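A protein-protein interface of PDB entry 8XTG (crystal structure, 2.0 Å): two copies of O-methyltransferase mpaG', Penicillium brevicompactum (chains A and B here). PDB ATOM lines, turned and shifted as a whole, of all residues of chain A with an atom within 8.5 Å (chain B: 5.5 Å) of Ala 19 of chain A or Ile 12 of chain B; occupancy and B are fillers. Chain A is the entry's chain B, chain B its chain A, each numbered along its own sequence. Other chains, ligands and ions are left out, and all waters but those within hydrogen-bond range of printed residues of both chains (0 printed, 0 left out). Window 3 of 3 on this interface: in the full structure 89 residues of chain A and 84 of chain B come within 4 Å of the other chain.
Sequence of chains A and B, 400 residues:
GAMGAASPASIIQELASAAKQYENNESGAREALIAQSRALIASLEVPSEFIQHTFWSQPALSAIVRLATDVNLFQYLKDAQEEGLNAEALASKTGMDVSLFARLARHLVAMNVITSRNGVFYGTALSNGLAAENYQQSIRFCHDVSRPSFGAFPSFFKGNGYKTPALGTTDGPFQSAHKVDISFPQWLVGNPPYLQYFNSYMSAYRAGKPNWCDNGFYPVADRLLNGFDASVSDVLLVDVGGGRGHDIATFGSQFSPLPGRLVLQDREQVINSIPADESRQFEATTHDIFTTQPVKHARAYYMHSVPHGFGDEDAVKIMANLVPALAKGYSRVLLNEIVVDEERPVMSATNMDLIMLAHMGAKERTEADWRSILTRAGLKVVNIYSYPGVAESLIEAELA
OG of Ser 37 of chain A sits at hydrogen-bond distance from O of Leu 33 of chain A (2.8 Å).
Among the printed residues, merely in contact across the chains: Ser 37 of chain A with Leu 40 of chain B, Ala 19 of chain A with Ile 12 of chain B, Tyr 22 of chain A with Pro 8 of chain B, Leu 33 of chain A with Ile 12 of chain B, Leu 15 of chain A with Leu 15 of chain B and Leu 33 of chain A with Leu 40 of chain B.
Ala 19 of chain A touches just one residue of chain B: Ile 12 (3.6 Å). Of chain A, only Ala 19 (3.6 Å) and Leu 33 (3.8 Å) come within 4 Å of Ile 12 of chain B. Printed residues of chain B within 4 Å of Leu 15 of chain A: Leu 15 (3.8 Å). Of the printed residues of chain A, Leu 40 of chain B touches Leu 33 and Ser 37. Of the printed residues of chain B, Ser 37 of chain A touches Leu 40 (3.3 Å). Ser 10 of chain B touches none of the printed residues of chain A. The nearest residue of chain A that does not touch Ile 12 of chain B is Tyr 22 of chain A (4.4 Å).
Printed residues of chain B that touch a printed residue of chain A: Pro 8, Ile 12, Leu 15 and Leu 40. Hydrophobic or aromatic side chains of chain B within 4 Å of the printed part of chain A: Pro 8, Ile 12, Leu 15 and Leu 40. Of the 22 printed residues of chain A, 5 touch a printed residue of chain B. Among the printed residues, 6 pairs touch across the chains. Among the printed residues, no Asp or Glu carboxylate lies within 4 Å of a Lys or Arg side-chain nitrogen of the other chain.
Leu 15 of chain A touches its own counterpart, Leu 15 of chain B. Positions printed for both chains: 12, 13, 14, 15, 16 and 17. Of the 6 pairs that touch across the chains among the printed residues, 1 has its exchanged pair printed and touching as well.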
ATOM      1  N   ILE A  12      28.069 -23.966  20.241  1.00  0.00           N
ATOM      2  CA  ILE A  12      28.022 -22.556  19.860  1.00  0.00           C
ATOM      3  C   ILE A  12      29.101 -22.255  18.826  1.00  0.00           C
ATOM      4  O   ILE A  12      28.889 -21.471  17.892  1.00  0.00           O
ATOM      5  CB  ILE A  12      28.160 -21.653  21.103  1.00  0.00           C
ATOM      6  CG1 ILE A  12      26.856 -21.618  21.900  1.00  0.00           C
ATOM      7  CG2 ILE A  12      28.529 -20.237  20.709  1.00  0.00           C
ATOM      8  CD1 ILE A  12      27.052 -21.729  23.399  1.00  0.00           C
ATOM      9  N   GLN A  13      30.267 -22.890  18.966  1.00  0.00           N
ATOM     10  CA  GLN A  13      31.348 -22.702  18.004  1.00  0.00           C
ATOM     11  C   GLN A  13      31.005 -23.335  16.660  1.00  0.00           C
ATOM     12  O   GLN A  13      31.176 -22.711  15.606  1.00  0.00           O
ATOM     13  CB  GLN A  13      32.639 -23.292  18.566  1.00  0.00           C
ATOM     14  CG  GLN A  13      33.232 -22.483  19.705  1.00  0.00           C
ATOM     15  CD  GLN A  13      34.684 -22.820  19.959  1.00  0.00           C
ATOM     16  OE1 GLN A  13      35.573 -21.990  19.758  1.00  0.00           O
ATOM     17  NE2 GLN A  13      34.936 -24.049  20.395  1.00  0.00           N
ATOM     18  N   GLU A  14      30.527 -24.582  16.677  1.00  0.00           N
ATOM     19  CA  GLU A  14      30.115 -25.239  15.440  1.00  0.00           C
ATOM     20  C   GLU A  14      28.969 -24.487  14.775  1.00  0.00           C
ATOM     21  O   GLU A  14      28.911 -24.387  13.544  1.00  0.00           O
ATOM     22  CB  GLU A  14      29.713 -26.686  15.726  1.00  0.00           C
ATOM     23  CG  GLU A  14      30.799 -27.725  15.470  1.00  0.00           C
ATOM     24  CD  GLU A  14      30.958 -28.086  13.995  1.00  0.00           C
ATOM     25  OE1 GLU A  14      30.534 -27.301  13.118  1.00  0.00           O
ATOM     26  OE2 GLU A  14      31.507 -29.171  13.712  1.00  0.00           O
ATOM     27  N   LEU A  15      28.045 -23.956  15.579  1.00  0.00           N
ATOM     28  CA  LEU A  15      26.928 -23.188  15.036  1.00  0.00           C
ATOM     29  C   LEU A  15      27.421 -21.940  14.309  1.00  0.00           C
ATOM     30  O   LEU A  15      26.936 -21.615  13.220  1.00  0.00           O
ATOM     31  CB  LEU A  15      25.963 -22.824  16.168  1.00  0.00           C
ATOM     32  CG  LEU A  15      24.555 -22.308  15.870  1.00  0.00           C
ATOM     33  CD1 LEU A  15      23.958 -23.055  14.718  1.00  0.00           C
ATOM     34  CD2 LEU A  15      23.677 -22.474  17.092  1.00  0.00           C
ATOM     35  N   ALA A  16      28.388 -21.230  14.896  1.00  0.00           N
ATOM     36  CA  ALA A  16      28.957 -20.064  14.226  1.00  0.00           C
ATOM     37  C   ALA A  16      29.780 -20.463  13.009  1.00  0.00           C
ATOM     38  O   ALA A  16      29.831 -19.714  12.028  1.00  0.00           O
ATOM     39  CB  ALA A  16      29.816 -19.256  15.198  1.00  0.00           C
ATOM     40  N   SER A  17      30.431 -21.628  13.054  1.00  0.00           N
ATOM     41  CA  SER A  17      31.155 -22.113  11.884  1.00  0.00           C
ATOM     42  C   SER A  17      30.196 -22.476  10.758  1.00  0.00           C
ATOM     43  O   SER A  17      30.469 -22.190   9.587  1.00  0.00           O
ATOM     44  CB  SER A  17      32.018 -23.314  12.262  1.00  0.00           C
ATOM     45  OG  SER A  17      32.552 -23.933  11.106  1.00  0.00           O
ATOM     46  N   ALA A  18      29.070 -23.109  11.093  1.00  0.00           N
ATOM     47  CA  ALA A  18      28.055 -23.401  10.086  1.00  0.00           C
ATOM     48  C   ALA A  18      27.436 -22.125   9.534  1.00  0.00           C
ATOM     49  O   ALA A  18      26.998 -22.101   8.377  1.00  0.00           O
ATOM     50  CB  ALA A  18      26.970 -24.301  10.674  1.00  0.00           C
ATOM     51  N   ALA A  19      27.395 -21.064  10.344  1.00  0.00           N
ATOM     52  CA  ALA A  19      26.834 -19.795   9.892  1.00  0.00           C
ATOM     53  C   ALA A  19      27.610 -19.249   8.703  1.00  0.00           C
ATOM     54  O   ALA A  19      27.030 -18.980   7.646  1.00  0.00           O
ATOM     55  CB  ALA A  19      26.821 -18.788  11.041  1.00  0.00           C
ATOM     56  N   LYS A  20      28.931 -19.101   8.854  1.00  0.00           N
ATOM     57  CA  LYS A  20      29.771 -18.589   7.772  1.00  0.00           C
ATOM     58  C   LYS A  20      29.545 -19.365   6.478  1.00  0.00           C
ATOM     59  O   LYS A  20      29.382 -18.775   5.404  1.00  0.00           O
ATOM     60  CB  LYS A  20      31.246 -18.659   8.173  1.00  0.00           C
ATOM     61  CG  LYS A  20      31.520 -18.377   9.636  1.00  0.00           C
ATOM     62  CD  LYS A  20      31.384 -16.904   9.965  1.00  0.00           C
ATOM     63  CE  LYS A  20      32.430 -16.481  10.992  1.00  0.00           C
ATOM     64  NZ  LYS A  20      31.885 -16.477  12.384  1.00  0.00           N
ATOM     65  N   GLN A  21      29.535 -20.698   6.570  1.00  0.00           N
ATOM     66  CA  GLN A  21      29.312 -21.533   5.396  1.00  0.00           C
ATOM     67  C   GLN A  21      27.959 -21.254   4.757  1.00  0.00           C
ATOM     68  O   GLN A  21      27.820 -21.347   3.532  1.00  0.00           O
ATOM     69  CB  GLN A  21      29.412 -23.004   5.789  1.00  0.00           C
ATOM     70  CG  GLN A  21      30.683 -23.355   6.532  1.00  0.00           C
ATOM     71  CD  GLN A  21      30.824 -24.843   6.748  1.00  0.00           C
ATOM     72  OE1 GLN A  21      30.063 -25.441   7.512  1.00  0.00           O
ATOM     73  NE2 GLN A  21      31.798 -25.452   6.081  1.00  0.00           N
ATOM     74  N   TYR A  22      26.955 -20.916   5.569  1.00  0.00           N
ATOM     75  CA  TYR A  22      25.638 -20.592   5.032  1.00  0.00           C
ATOM     76  C   TYR A  22      25.638 -19.220   4.362  1.00  0.00           C
ATOM     77  O   TYR A  22      25.008 -19.037   3.313  1.00  0.00           O
ATOM     78  CB  TYR A  22      24.592 -20.661   6.148  1.00  0.00           C
ATOM     79  CG  TYR A  22      23.249 -20.066   5.784  1.00  0.00           C
ATOM     80  CD1 TYR A  22      22.375 -20.742   4.945  1.00  0.00           C
ATOM     81  CD2 TYR A  22      22.857 -18.829   6.280  1.00  0.00           C
ATOM     82  CE1 TYR A  22      21.150 -20.206   4.609  1.00  0.00           C
ATOM     83  CE2 TYR A  22      21.635 -18.283   5.947  1.00  0.00           C
ATOM     84  CZ  TYR A  22      20.786 -18.976   5.110  1.00  0.00           C
ATOM     85  OH  TYR A  22      19.563 -18.439   4.777  1.00  0.00           O
ATOM     86  N   GLU A  23      26.342 -18.244   4.947  1.00  0.00           N
ATOM     87  CA  GLU A  23      26.472 -16.943   4.295  1.00  0.00           C
ATOM     88  C   GLU A  23      27.240 -17.062   2.986  1.00  0.00           C
ATOM     89  O   GLU A  23      26.951 -16.348   2.020  1.00  0.00           O
ATOM     90  CB  GLU A  23      27.159 -15.940   5.226  1.00  0.00           C
ATOM     91  CG  GLU A  23      26.937 -16.202   6.703  1.00  0.00           C
ATOM     92  CD  GLU A  23      27.409 -15.070   7.596  1.00  0.00           C
ATOM     93  OE1 GLU A  23      28.610 -14.723   7.537  1.00  0.00           O
ATOM     94  OE2 GLU A  23      26.582 -14.544   8.373  1.00  0.00           O
ATOM     95  N   ASN A  24      28.222 -17.959   2.937  1.00  0.00           N
ATOM     96  CA  ASN A  24      28.989 -18.220   1.726  1.00  0.00           C
ATOM     97  C   ASN A  24      28.239 -19.121   0.744  1.00  0.00           C
ATOM     98  O   ASN A  24      28.825 -19.573  -0.246  1.00  0.00           O
ATOM     99  CB  ASN A  24      30.349 -18.826   2.103  1.00  0.00           C
ATOM    100  CG  ASN A  24      31.320 -18.880   0.936  1.00  0.00           C
ATOM    101  OD1 ASN A  24      31.508 -19.928   0.318  1.00  0.00           O
ATOM    102  ND2 ASN A  24      31.936 -17.745   0.624  1.00  0.00           N
ATOM    103  N   ASN A  25      26.955 -19.386   0.999  1.00  0.00           N
ATOM    104  CA  ASN A  25      26.081 -20.146   0.104  1.00  0.00           C
ATOM    105  C   ASN A  25      26.600 -21.558  -0.162  1.00  0.00           C
ATOM    106  O   ASN A  25      26.253 -22.170  -1.177  1.00  0.00           O
ATOM    107  CB  ASN A  25      25.865 -19.399  -1.219  1.00  0.00           C
ATOM    108  CG  ASN A  25      24.569 -19.789  -1.908  1.00  0.00           C
ATOM    109  OD1 ASN A  25      23.481 -19.405  -1.476  1.00  0.00           O
ATOM    110  ND2 ASN A  25      24.682 -20.544  -2.995  1.00  0.00           N
ATOM    111  N   GLU A  26      27.424 -22.092   0.736  1.00  0.00           N
ATOM    112  CA  GLU A  26      27.948 -23.437   0.553  1.00  0.00           C
ATOM    113  C   GLU A  26      26.821 -24.454   0.672  1.00  0.00           C
ATOM    114  O   GLU A  26      25.939 -24.331   1.525  1.00  0.00           O
ATOM    115  CB  GLU A  26      29.045 -23.724   1.578  1.00  0.00           C
ATOM    116  CG  GLU A  26      30.192 -22.724   1.535  1.00  0.00           C
ATOM    117  CD  GLU A  26      31.358 -23.119   2.424  1.00  0.00           C
ATOM    118  OE1 GLU A  26      31.371 -24.266   2.920  1.00  0.00           O
ATOM    119  OE2 GLU A  26      32.261 -22.277   2.626  1.00  0.00           O
ATOM    120  N   ALA A  29      24.932 -26.223   3.904  1.00  0.00           N
ATOM    121  CA  ALA A  29      25.201 -25.459   5.119  1.00  0.00           C
ATOM    122  C   ALA A  29      23.920 -25.013   5.812  1.00  0.00           C
ATOM    123  O   ALA A  29      23.878 -24.945   7.047  1.00  0.00           O
ATOM    124  CB  ALA A  29      26.079 -24.250   4.791  1.00  0.00           C
ATOM    125  N   ARG A  30      22.870 -24.704   5.045  1.00  0.00           N
ATOM    126  CA  ARG A  30      21.591 -24.344   5.649  1.00  0.00           C
ATOM    127  C   ARG A  30      21.075 -25.469   6.538  1.00  0.00           C
ATOM    128  O   ARG A  30      20.664 -25.236   7.679  1.00  0.00           O
ATOM    129  CB  ARG A  30      20.574 -24.000   4.560  1.00  0.00           C
ATOM    130  CG  ARG A  30      19.207 -23.566   5.087  1.00  0.00           C
ATOM    131  CD  ARG A  30      18.224 -23.325   3.943  1.00  0.00           C
ATOM    132  NE  ARG A  30      17.899 -24.551   3.226  1.00  0.00           N
ATOM    133  CZ  ARG A  30      17.151 -25.534   3.711  1.00  0.00           C
ATOM    134  NH1 ARG A  30      16.560 -25.438   4.892  1.00  0.00           N
ATOM    135  NH2 ARG A  30      16.983 -26.639   2.988  1.00  0.00           N
ATOM    136  N   ALA A  32      22.920 -27.798   7.859  1.00  0.00           N
ATOM    137  CA  ALA A  32      23.855 -27.956   8.970  1.00  0.00           C
ATOM    138  C   ALA A  32      23.643 -26.889  10.036  1.00  0.00           C
ATOM    139  O   ALA A  32      23.840 -27.155  11.228  1.00  0.00           O
ATOM    140  CB  ALA A  32      25.293 -27.917   8.457  1.00  0.00           C
ATOM    141  N   LEU A  33      23.261 -25.676   9.628  1.00  0.00           N
ATOM    142  CA  LEU A  33      22.886 -24.650  10.594  1.00  0.00           C
ATOM    143  C   LEU A  33      21.654 -25.080  11.385  1.00  0.00           C
ATOM    144  O   LEU A  33      21.582 -24.880  12.606  1.00  0.00           O
ATOM    145  CB  LEU A  33      22.635 -23.330   9.863  1.00  0.00           C
ATOM    146  CG  LEU A  33      22.800 -22.000  10.594  1.00  0.00           C
ATOM    147  CD1 LEU A  33      24.057 -22.016  11.428  1.00  0.00           C
ATOM    148  CD2 LEU A  33      22.837 -20.848   9.604  1.00  0.00           C
ATOM    149  N   ILE A  34      20.676 -25.686  10.703  1.00  0.00           N
ATOM    150  CA  ILE A  34      19.506 -26.248  11.376  1.00  0.00           C
ATOM    151  C   ILE A  34      19.918 -27.360  12.334  1.00  0.00           C
ATOM    152  O   ILE A  34      19.388 -27.467  13.447  1.00  0.00           O
ATOM    153  CB  ILE A  34      18.485 -26.741  10.331  1.00  0.00           C
ATOM    154  CG1 ILE A  34      17.979 -25.572   9.484  1.00  0.00           C
ATOM    155  CG2 ILE A  34      17.322 -27.471  10.995  1.00  0.00           C
ATOM    156  CD1 ILE A  34      17.314 -25.993   8.199  1.00  0.00           C
ATOM    157  N   GLN A  36      22.970 -27.855  13.829  1.00  0.00           N
ATOM    158  CA  GLN A  36      23.694 -27.321  14.979  1.00  0.00           C
ATOM    159  C   GLN A  36      22.761 -26.581  15.936  1.00  0.00           C
ATOM    160  O   GLN A  36      22.990 -26.593  17.152  1.00  0.00           O
ATOM    161  CB  GLN A  36      24.822 -26.404  14.505  1.00  0.00           C
ATOM    162  CG  GLN A  36      26.033 -27.128  13.928  1.00  0.00           C
ATOM    163  CD  GLN A  36      26.524 -28.252  14.820  1.00  0.00           C
ATOM    164  OE1 GLN A  36      26.640 -28.091  16.037  1.00  0.00           O
ATOM    165  NE2 GLN A  36      26.818 -29.399  14.218  1.00  0.00           N
ATOM    166  N   SER A  37      21.709 -25.944  15.415  1.00  0.00           N
ATOM    167  CA  SER A  37      20.740 -25.279  16.283  1.00  0.00           C
ATOM    168  C   SER A  37      20.028 -26.282  17.184  1.00  0.00           C
ATOM    169  O   SER A  37      19.840 -26.032  18.380  1.00  0.00           O
ATOM    170  CB  SER A  37      19.719 -24.508  15.446  1.00  0.00           C
ATOM    171  OG  SER A  37      20.330 -23.475  14.691  1.00  0.00           O
ATOM    172  N   SER B   7      15.438 -11.892   9.531  1.00  0.00           N
ATOM    173  CA  SER B   7      16.428 -12.486   8.637  1.00  0.00           C
ATOM    174  C   SER B   7      17.289 -13.504   9.375  1.00  0.00           C
ATOM    175  O   SER B   7      17.598 -13.320  10.556  1.00  0.00           O
ATOM    176  CB  SER B   7      17.311 -11.399   8.018  1.00  0.00           C
ATOM    177  OG  SER B   7      18.554 -11.302   8.692  1.00  0.00           O
ATOM    178  N   PRO B   8      17.665 -14.586   8.685  1.00  0.00           N
ATOM    179  CA  PRO B   8      18.558 -15.570   9.317  1.00  0.00           C
ATOM    180  C   PRO B   8      19.827 -14.945   9.871  1.00  0.00           C
ATOM    181  O   PRO B   8      20.190 -15.220  11.019  1.00  0.00           O
ATOM    182  CB  PRO B   8      18.844 -16.561   8.178  1.00  0.00           C
ATOM    183  CG  PRO B   8      17.654 -16.453   7.285  1.00  0.00           C
ATOM    184  CD  PRO B   8      17.258 -14.997   7.330  1.00  0.00           C
ATOM    185  N   ALA B   9      20.489 -14.078   9.097  1.00  0.00           N
ATOM    186  CA  ALA B   9      21.718 -13.446   9.571  1.00  0.00           C
ATOM    187  C   ALA B   9      21.483 -12.658  10.855  1.00  0.00           C
ATOM    188  O   ALA B   9      22.328 -12.665  11.757  1.00  0.00           O
ATOM    189  CB  ALA B   9      22.297 -12.541   8.485  1.00  0.00           C
ATOM    190  N   SER B  10      20.338 -11.977  10.960  1.00  0.00           N
ATOM    191  CA  SER B  10      19.999 -11.265  12.189  1.00  0.00           C
ATOM    192  C   SER B  10      19.924 -12.218  13.377  1.00  0.00           C
ATOM    193  O   SER B  10      20.521 -11.966  14.431  1.00  0.00           O
ATOM    194  CB  SER B  10      18.674 -10.523  12.013  1.00  0.00           C
ATOM    195  OG  SER B  10      17.973 -10.438  13.243  1.00  0.00           O
ATOM    196  N   ILE B  11      19.186 -13.322  13.222  1.00  0.00           N
ATOM    197  CA  ILE B  11      19.048 -14.301  14.297  1.00  0.00           C
ATOM    198  C   ILE B  11      20.391 -14.935  14.633  1.00  0.00           C
ATOM    199  O   ILE B  11      20.664 -15.249  15.799  1.00  0.00           O
ATOM    200  CB  ILE B  11      17.994 -15.361  13.910  1.00  0.00           C
ATOM    201  CG1 ILE B  11      16.705 -14.678  13.441  1.00  0.00           C
ATOM    202  CG2 ILE B  11      17.726 -16.315  15.066  1.00  0.00           C
ATOM    203  CD1 ILE B  11      15.600 -15.640  13.072  1.00  0.00           C
ATOM    204  N   ILE B  12      21.251 -15.130  13.630  1.00  0.00           N
ATOM    205  CA  ILE B  12      22.583 -15.671  13.884  1.00  0.00           C
ATOM    206  C   ILE B  12      23.389 -14.746  14.796  1.00  0.00           C
ATOM    207  O   ILE B  12      24.118 -15.212  15.678  1.00  0.00           O
ATOM    208  CB  ILE B  12      23.316 -15.949  12.557  1.00  0.00           C
ATOM    209  CG1 ILE B  12      22.549 -16.971  11.713  1.00  0.00           C
ATOM    210  CG2 ILE B  12      24.729 -16.427  12.813  1.00  0.00           C
ATOM    211  CD1 ILE B  12      23.119 -17.177  10.326  1.00  0.00           C
ATOM    212  N   GLN B  13      23.279 -13.426  14.603  1.00  0.00           N
ATOM    213  CA  GLN B  13      24.026 -12.501  15.456  1.00  0.00           C
ATOM    214  C   GLN B  13      23.401 -12.411  16.829  1.00  0.00           C
ATOM    215  O   GLN B  13      24.102 -12.331  17.853  1.00  0.00           O
ATOM    216  CB  GLN B  13      24.078 -11.110  14.828  1.00  0.00           C
ATOM    217  CG  GLN B  13      24.415 -11.100  13.351  1.00  0.00           C
ATOM    218  CD  GLN B  13      24.449  -9.700  12.761  1.00  0.00           C
ATOM    219  OE1 GLN B  13      23.417  -9.038  12.627  1.00  0.00           O
ATOM    220  NE2 GLN B  13      25.649  -9.230  12.435  1.00  0.00           N
ATOM    221  N   GLU B  14      22.078 -12.401  16.857  1.00  0.00           N
ATOM    222  CA  GLU B  14      21.376 -12.391  18.119  1.00  0.00           C
ATOM    223  C   GLU B  14      21.661 -13.658  18.939  1.00  0.00           C
ATOM    224  O   GLU B  14      21.964 -13.552  20.129  1.00  0.00           O
ATOM    225  CB  GLU B  14      19.886 -12.155  17.820  1.00  0.00           C
ATOM    226  CG  GLU B  14      19.058 -12.323  19.036  1.00  0.00           C
ATOM    227  CD  GLU B  14      19.632 -11.543  20.193  1.00  0.00           C
ATOM    228  OE1 GLU B  14      19.798 -10.335  20.006  1.00  0.00           O
ATOM    229  OE2 GLU B  14      19.910 -12.115  21.279  1.00  0.00           O
ATOM    230  N   LEU B  15      21.711 -14.834  18.298  1.00  0.00           N
ATOM    231  CA  LEU B  15      22.104 -16.063  18.994  1.00  0.00           C
ATOM    232  C   LEU B  15      23.492 -15.953  19.640  1.00  0.00           C
ATOM    233  O   LEU B  15      23.692 -16.383  20.787  1.00  0.00           O
ATOM    234  CB  LEU B  15      22.059 -17.229  18.007  1.00  0.00           C
ATOM    235  CG  LEU B  15      21.937 -18.645  18.558  1.00  0.00           C
ATOM    236  CD1 LEU B  15      21.248 -19.514  17.516  1.00  0.00           C
ATOM    237  CD2 LEU B  15      23.290 -19.216  18.918  1.00  0.00           C
ATOM    238  N   ALA B  16      24.468 -15.395  18.918  1.00  0.00           N
ATOM    239  CA  ALA B  16      25.809 -15.241  19.475  1.00  0.00           C
ATOM    240  C   ALA B  16      25.831 -14.260  20.644  1.00  0.00           C
ATOM    241  O   ALA B  16      26.630 -14.426  21.574  1.00  0.00           O
ATOM    242  CB  ALA B  16      26.783 -14.792  18.385  1.00  0.00           C
ATOM    243  N   SER B  17      24.973 -13.237  20.616  1.00  0.00           N
ATOM    244  CA  SER B  17      24.879 -12.322  21.749  1.00  0.00           C
ATOM    245  C   SER B  17      24.358 -13.040  22.989  1.00  0.00           C
ATOM    246  O   SER B  17      24.966 -12.968  24.062  1.00  0.00           O
ATOM    247  CB  SER B  17      23.981 -11.137  21.396  1.00  0.00           C
ATOM    248  OG  SER B  17      23.510 -10.492  22.567  1.00  0.00           O
ATOM    249  N   LEU B  40      15.999 -19.480  14.750  1.00  0.00           N
ATOM    250  CA  LEU B  40      16.882 -19.743  13.621  1.00  0.00           C
ATOM    251  C   LEU B  40      16.382 -20.918  12.786  1.00  0.00           C
ATOM    252  O   LEU B  40      16.400 -20.858  11.551  1.00  0.00           O
ATOM    253  CB  LEU B  40      18.308 -20.002  14.112  1.00  0.00           C
ATOM    254  CG  LEU B  40      19.367 -20.103  13.010  1.00  0.00           C
ATOM    255  CD1 LEU B  40      19.357 -18.859  12.126  1.00  0.00           C
ATOM    256  CD2 LEU B  40      20.750 -20.346  13.600  1.00  0.00           C
